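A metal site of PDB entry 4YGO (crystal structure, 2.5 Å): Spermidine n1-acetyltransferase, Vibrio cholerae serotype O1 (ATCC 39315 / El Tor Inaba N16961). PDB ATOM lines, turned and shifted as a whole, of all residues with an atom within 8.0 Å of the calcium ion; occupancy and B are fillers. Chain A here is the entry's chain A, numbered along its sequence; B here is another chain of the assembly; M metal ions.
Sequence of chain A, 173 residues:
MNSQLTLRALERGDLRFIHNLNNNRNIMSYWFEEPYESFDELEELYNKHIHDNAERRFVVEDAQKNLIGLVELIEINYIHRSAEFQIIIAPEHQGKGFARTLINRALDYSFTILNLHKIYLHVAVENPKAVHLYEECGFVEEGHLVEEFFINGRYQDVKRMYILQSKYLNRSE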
ATOM      1  N   PHE A  32      24.191  28.188 -11.686  1.00  0.00           N
ATOM      2  CA  PHE A  32      25.319  27.206 -11.563  1.00  0.00           C
ATOM      3  C   PHE A  32      26.150  27.368 -10.293  1.00  0.00           C
ATOM      4  O   PHE A  32      27.371  27.282 -10.279  1.00  0.00           O
ATOM      5  CB  PHE A  32      26.180  27.164 -12.820  1.00  0.00           C
ATOM      6  CG  PHE A  32      25.472  26.589 -13.992  1.00  0.00           C
ATOM      7  CD1 PHE A  32      24.520  27.347 -14.673  1.00  0.00           C
ATOM      8  CD2 PHE A  32      25.732  25.281 -14.427  1.00  0.00           C
ATOM      9  CE1 PHE A  32      23.847  26.866 -15.777  1.00  0.00           C
ATOM     10  CE2 PHE A  32      25.064  24.777 -15.551  1.00  0.00           C
ATOM     11  CZ  PHE A  32      24.111  25.572 -16.212  1.00  0.00           C
ATOM     12  N   GLU A  33      25.420  27.575  -9.195  1.00  0.00           N
ATOM     13  CA  GLU A  33      25.986  27.680  -7.841  1.00  0.00           C
ATOM     14  C   GLU A  33      26.718  29.004  -7.581  1.00  0.00           C
ATOM     15  O   GLU A  33      27.166  29.232  -6.451  1.00  0.00           O
ATOM     16  CB  GLU A  33      26.769  26.404  -7.430  1.00  0.00           C
ATOM     17  CG  GLU A  33      25.849  25.192  -7.639  1.00  0.00           C
ATOM     18  CD  GLU A  33      26.320  23.890  -7.018  1.00  0.00           C
ATOM     19  OE1 GLU A  33      26.676  23.903  -5.805  1.00  0.00           O
ATOM     20  OE2 GLU A  33      26.254  22.848  -7.740  1.00  0.00           O
ATOM     21  N   ALA A  54      24.977  20.505 -15.999  1.00  0.00           N
ATOM     22  CA  ALA A  54      24.575  20.343 -14.584  1.00  0.00           C
ATOM     23  C   ALA A  54      23.258  21.008 -14.205  1.00  0.00           C
ATOM     24  O   ALA A  54      22.755  20.756 -13.120  1.00  0.00           O
ATOM     25  CB  ALA A  54      25.667  20.830 -13.624  1.00  0.00           C
ATOM     26  N   GLU A  55      22.757  21.888 -15.055  1.00  0.00           N
ATOM     27  CA  GLU A  55      21.481  22.583 -14.804  1.00  0.00           C
ATOM     28  C   GLU A  55      20.781  22.779 -16.139  1.00  0.00           C
ATOM     29  O   GLU A  55      21.465  22.901 -17.183  1.00  0.00           O
ATOM     30  CB  GLU A  55      21.700  23.948 -14.132  1.00  0.00           C
ATOM     31  CG  GLU A  55      22.374  23.847 -12.786  1.00  0.00           C
ATOM     32  CD  GLU A  55      22.486  25.171 -12.029  1.00  0.00           C
ATOM     33  OE1 GLU A  55      22.999  25.109 -10.912  1.00  0.00           O
ATOM     34  OE2 GLU A  55      22.090  26.265 -12.531  1.00  0.00           O
ATOM     35  N   ILE A  74      18.402  21.376 -11.278  1.00  0.00           N
ATOM     36  CA  ILE A  74      19.808  21.608 -10.909  1.00  0.00           C
ATOM     37  C   ILE A  74      20.382  20.381 -10.233  1.00  0.00           C
ATOM     38  O   ILE A  74      19.651  19.438  -9.924  1.00  0.00           O
ATOM     39  CB  ILE A  74      19.990  22.893 -10.031  1.00  0.00           C
ATOM     40  CG1 ILE A  74      19.483  22.724  -8.595  1.00  0.00           C
ATOM     41  CG2 ILE A  74      19.245  24.110 -10.638  1.00  0.00           C
ATOM     42  CD1 ILE A  74      19.577  24.024  -7.796  1.00  0.00           C
ATOM     43  N   GLU A  75      21.702  20.405 -10.008  1.00  0.00           N
ATOM     44  CA  GLU A  75      22.403  19.296  -9.384  1.00  0.00           C
ATOM     45  C   GLU A  75      22.193  17.992 -10.163  1.00  0.00           C
ATOM     46  O   GLU A  75      22.110  16.972  -9.598  1.00  0.00           O
ATOM     47  CB  GLU A  75      21.949  19.098  -7.918  1.00  0.00           C
ATOM     48  CG  GLU A  75      22.270  20.251  -6.985  1.00  0.00           C
ATOM     49  CD  GLU A  75      23.737  20.327  -6.591  1.00  0.00           C
ATOM     50  OE1 GLU A  75      24.542  19.457  -6.990  1.00  0.00           O
ATOM     51  OE2 GLU A  75      24.067  21.238  -5.835  1.00  0.00           O
ATOM     52  N   ILE A  76      22.122  18.067 -11.467  1.00  0.00           N
ATOM     53  CA  ILE A  76      21.941  16.899 -12.321  1.00  0.00           C
ATOM     54  C   ILE A  76      23.238  16.073 -12.313  1.00  0.00           C
ATOM     55  O   ILE A  76      24.337  16.540 -12.655  1.00  0.00           O
ATOM     56  CB  ILE A  76      21.623  17.273 -13.763  1.00  0.00           C
ATOM     57  CG1 ILE A  76      20.372  18.151 -13.835  1.00  0.00           C
ATOM     58  CG2 ILE A  76      21.326  16.029 -14.552  1.00  0.00           C
ATOM     59  CD1 ILE A  76      20.202  18.846 -15.179  1.00  0.00           C
ATOM     60  N   GLU A  84      17.668  17.959  -8.742  1.00  0.00           N
ATOM     61  CA  GLU A  84      16.826  18.654  -7.822  1.00  0.00           C
ATOM     62  C   GLU A  84      15.927  19.519  -8.654  1.00  0.00           C
ATOM     63  O   GLU A  84      16.330  20.049  -9.719  1.00  0.00           O
ATOM     64  CB  GLU A  84      17.625  19.543  -6.919  1.00  0.00           C
ATOM     65  CG  GLU A  84      16.746  20.545  -6.170  1.00  0.00           C
ATOM     66  CD  GLU A  84      17.483  21.294  -5.080  1.00  0.00           C
ATOM     67  OE1 GLU A  84      18.703  21.101  -4.943  1.00  0.00           O
ATOM     68  OE2 GLU A  84      16.823  22.073  -4.366  1.00  0.00           O
ATOM     69  N   TYR A 120      14.066  15.197  -6.904  1.00  0.00           N
ATOM     70  CA  TYR A 120      13.669  15.648  -5.562  1.00  0.00           C
ATOM     71  C   TYR A 120      13.539  17.183  -5.464  1.00  0.00           C
ATOM     72  O   TYR A 120      14.004  17.913  -6.343  1.00  0.00           O
ATOM     73  CB  TYR A 120      14.631  15.064  -4.539  1.00  0.00           C
ATOM     74  CG  TYR A 120      15.993  15.513  -4.757  1.00  0.00           C
ATOM     75  CD1 TYR A 120      16.446  16.708  -4.192  1.00  0.00           C
ATOM     76  CD2 TYR A 120      16.874  14.781  -5.549  1.00  0.00           C
ATOM     77  CE1 TYR A 120      17.767  17.161  -4.418  1.00  0.00           C
ATOM     78  CE2 TYR A 120      18.212  15.221  -5.781  1.00  0.00           C
ATOM     79  CZ  TYR A 120      18.633  16.410  -5.230  1.00  0.00           C
ATOM     80  OH  TYR A 120      19.904  16.870  -5.436  1.00  0.00           O
ATOM     81  N   PHE B  32      35.125  18.813  -7.830  1.00  0.00           N
ATOM     82  CA  PHE B  32      34.176  19.948  -8.083  1.00  0.00           C
ATOM     83  C   PHE B  32      33.033  19.579  -9.032  1.00  0.00           C
ATOM     84  O   PHE B  32      32.731  20.269  -9.974  1.00  0.00           O
ATOM     85  CB  PHE B  32      34.913  21.209  -8.529  1.00  0.00           C
ATOM     86  CG  PHE B  32      35.735  21.853  -7.442  1.00  0.00           C
ATOM     87  CD1 PHE B  32      36.966  21.298  -7.040  1.00  0.00           C
ATOM     88  CD2 PHE B  32      35.332  23.066  -6.829  1.00  0.00           C
ATOM     89  CE1 PHE B  32      37.727  21.868  -6.050  1.00  0.00           C
ATOM     90  CE2 PHE B  32      36.120  23.658  -5.840  1.00  0.00           C
ATOM     91  CZ  PHE B  32      37.316  23.053  -5.451  1.00  0.00           C
ATOM     92  N   GLU B  33      32.458  18.408  -8.765  1.00  0.00           N
ATOM     93  CA  GLU B  33      31.306  17.870  -9.511  1.00  0.00           C
ATOM     94  C   GLU B  33      31.643  17.419 -10.938  1.00  0.00           C
ATOM     95  O   GLU B  33      30.744  17.010 -11.650  1.00  0.00           O
ATOM     96  CB  GLU B  33      30.063  18.823  -9.444  1.00  0.00           C
ATOM     97  CG  GLU B  33      29.853  19.320  -8.009  1.00  0.00           C
ATOM     98  CD  GLU B  33      28.487  19.844  -7.677  1.00  0.00           C
ATOM     99  OE1 GLU B  33      27.508  19.069  -7.764  1.00  0.00           O
ATOM    100  OE2 GLU B  33      28.372  21.002  -7.215  1.00  0.00           O
ATOM    101  N   ALA B  54      34.167  26.455  -3.242  1.00  0.00           N
ATOM    102  CA  ALA B  54      33.034  25.590  -3.038  1.00  0.00           C
ATOM    103  C   ALA B  54      33.375  24.228  -2.438  1.00  0.00           C
ATOM    104  O   ALA B  54      32.456  23.554  -1.961  1.00  0.00           O
ATOM    105  CB  ALA B  54      32.311  25.368  -4.348  1.00  0.00           C
ATOM    106  N   GLU B  55      34.642  23.812  -2.492  1.00  0.00           N
ATOM    107  CA  GLU B  55      35.063  22.552  -1.887  1.00  0.00           C
ATOM    108  C   GLU B  55      36.422  22.744  -1.277  1.00  0.00           C
ATOM    109  O   GLU B  55      37.235  23.556  -1.780  1.00  0.00           O
ATOM    110  CB  GLU B  55      35.095  21.395  -2.908  1.00  0.00           C
ATOM    111  CG  GLU B  55      33.913  21.337  -3.859  1.00  0.00           C
ATOM    112  CD  GLU B  55      33.846  20.059  -4.673  1.00  0.00           C
ATOM    113  OE1 GLU B  55      32.756  19.686  -5.154  1.00  0.00           O
ATOM    114  OE2 GLU B  55      34.886  19.415  -4.885  1.00  0.00           O
ATOM    115  N   ILE B  74      32.354  19.543   0.781  1.00  0.00           N
ATOM    116  CA  ILE B  74      31.864  20.018  -0.546  1.00  0.00           C
ATOM    117  C   ILE B  74      30.514  20.701  -0.408  1.00  0.00           C
ATOM    118  O   ILE B  74      29.971  20.716   0.661  1.00  0.00           O
ATOM    119  CB  ILE B  74      31.839  18.877  -1.582  1.00  0.00           C
ATOM    120  CG1 ILE B  74      30.856  17.813  -1.230  1.00  0.00           C
ATOM    121  CG2 ILE B  74      33.209  18.196  -1.684  1.00  0.00           C
ATOM    122  CD1 ILE B  74      30.772  16.761  -2.298  1.00  0.00           C
ATOM    123  N   GLU B  75      30.015  21.266  -1.504  1.00  0.00           N
ATOM    124  CA  GLU B  75      28.791  22.093  -1.546  1.00  0.00           C
ATOM    125  C   GLU B  75      28.815  23.155  -0.472  1.00  0.00           C
ATOM    126  O   GLU B  75      27.900  23.308   0.250  1.00  0.00           O
ATOM    127  CB  GLU B  75      27.550  21.214  -1.343  1.00  0.00           C
ATOM    128  CG  GLU B  75      27.358  20.148  -2.383  1.00  0.00           C
ATOM    129  CD  GLU B  75      26.963  20.663  -3.732  1.00  0.00           C
ATOM    130  OE1 GLU B  75      26.495  21.823  -3.846  1.00  0.00           O
ATOM    131  OE2 GLU B  75      27.084  19.872  -4.685  1.00  0.00           O
ATOM    132  N   ILE B  76      29.895  23.888  -0.340  1.00  0.00           N
ATOM    133  CA  ILE B  76      29.970  24.869   0.701  1.00  0.00           C
ATOM    134  C   ILE B  76      29.167  26.068   0.200  1.00  0.00           C
ATOM    135  O   ILE B  76      29.356  26.531  -0.929  1.00  0.00           O
ATOM    136  CB  ILE B  76      31.387  25.287   0.994  1.00  0.00           C
ATOM    137  CG1 ILE B  76      32.203  24.050   1.312  1.00  0.00           C
ATOM    138  CG2 ILE B  76      31.401  26.208   2.213  1.00  0.00           C
ATOM    139  CD1 ILE B  76      33.652  24.353   1.495  1.00  0.00           C
ATOM    140  N   GLU B  84      28.613  19.731   2.918  1.00  0.00           N
ATOM    141  CA  GLU B  84      28.516  18.283   2.922  1.00  0.00           C
ATOM    142  C   GLU B  84      29.898  17.787   3.296  1.00  0.00           C
ATOM    143  O   GLU B  84      30.861  18.318   2.852  1.00  0.00           O
ATOM    144  CB  GLU B  84      28.122  17.704   1.569  1.00  0.00           C
ATOM    145  CG  GLU B  84      28.084  16.176   1.639  1.00  0.00           C
ATOM    146  CD  GLU B  84      27.638  15.489   0.366  1.00  0.00           C
ATOM    147  OE1 GLU B  84      26.958  16.131  -0.500  1.00  0.00           O
ATOM    148  OE2 GLU B  84      27.955  14.263   0.312  1.00  0.00           O
ATOM    149  N   TYR B 120      26.576  18.357   7.110  1.00  0.00           N
ATOM    150  CA  TYR B 120      25.842  17.110   6.946  1.00  0.00           C
ATOM    151  C   TYR B 120      26.655  16.096   6.183  1.00  0.00           C
ATOM    152  O   TYR B 120      27.610  16.434   5.561  1.00  0.00           O
ATOM    153  CB  TYR B 120      24.461  17.363   6.282  1.00  0.00           C
ATOM    154  CG  TYR B 120      24.574  17.995   4.957  1.00  0.00           C
ATOM    155  CD1 TYR B 120      24.627  19.386   4.834  1.00  0.00           C
ATOM    156  CD2 TYR B 120      24.645  17.236   3.825  1.00  0.00           C
ATOM    157  CE1 TYR B 120      24.773  19.990   3.602  1.00  0.00           C
ATOM    158  CE2 TYR B 120      24.785  17.819   2.573  1.00  0.00           C
ATOM    159  CZ  TYR B 120      24.863  19.189   2.465  1.00  0.00           C
ATOM    160  OH  TYR B 120      25.019  19.753   1.227  1.00  0.00           O
HETATM  161 CA    CA M   1      26.323  21.038  -6.337  1.00  0.00          CA
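O of Ala 54 of chain B is in hydrogen-bond range of N of Glu 75 of chain B (3.4 Å). The backbone carbonyl oxygen (O) of Ala 54 of chain A sits at hydrogen-bond distance from the backbone NH (N) of Glu 75 of chain A, 3.3 Å away.
Of the 18 residues printed, 4 come within 4 Å of the calcium ion.
The calcium ion is bound by OE2 of Glu 75 of chain B (2.2 Å), OE2 of Glu 33 of chain B (2.2 Å), OE2 of Glu 33 of chain A (2.3 Å), OE2 of Glu 75 of chain A (2.3 Å), OE1 of Glu 75 of chain A (2.5 Å), OE1 of Glu 75 of chain B (2.6 Å) and OE1 of Glu 33 of chain B (2.7 Å). The calcium ion has seven donor atoms within binding distance. Slightly farther from the calcium ion lies the side-chain carboxylate (OE1) of Glu 33 of chain A (2.9 Å).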
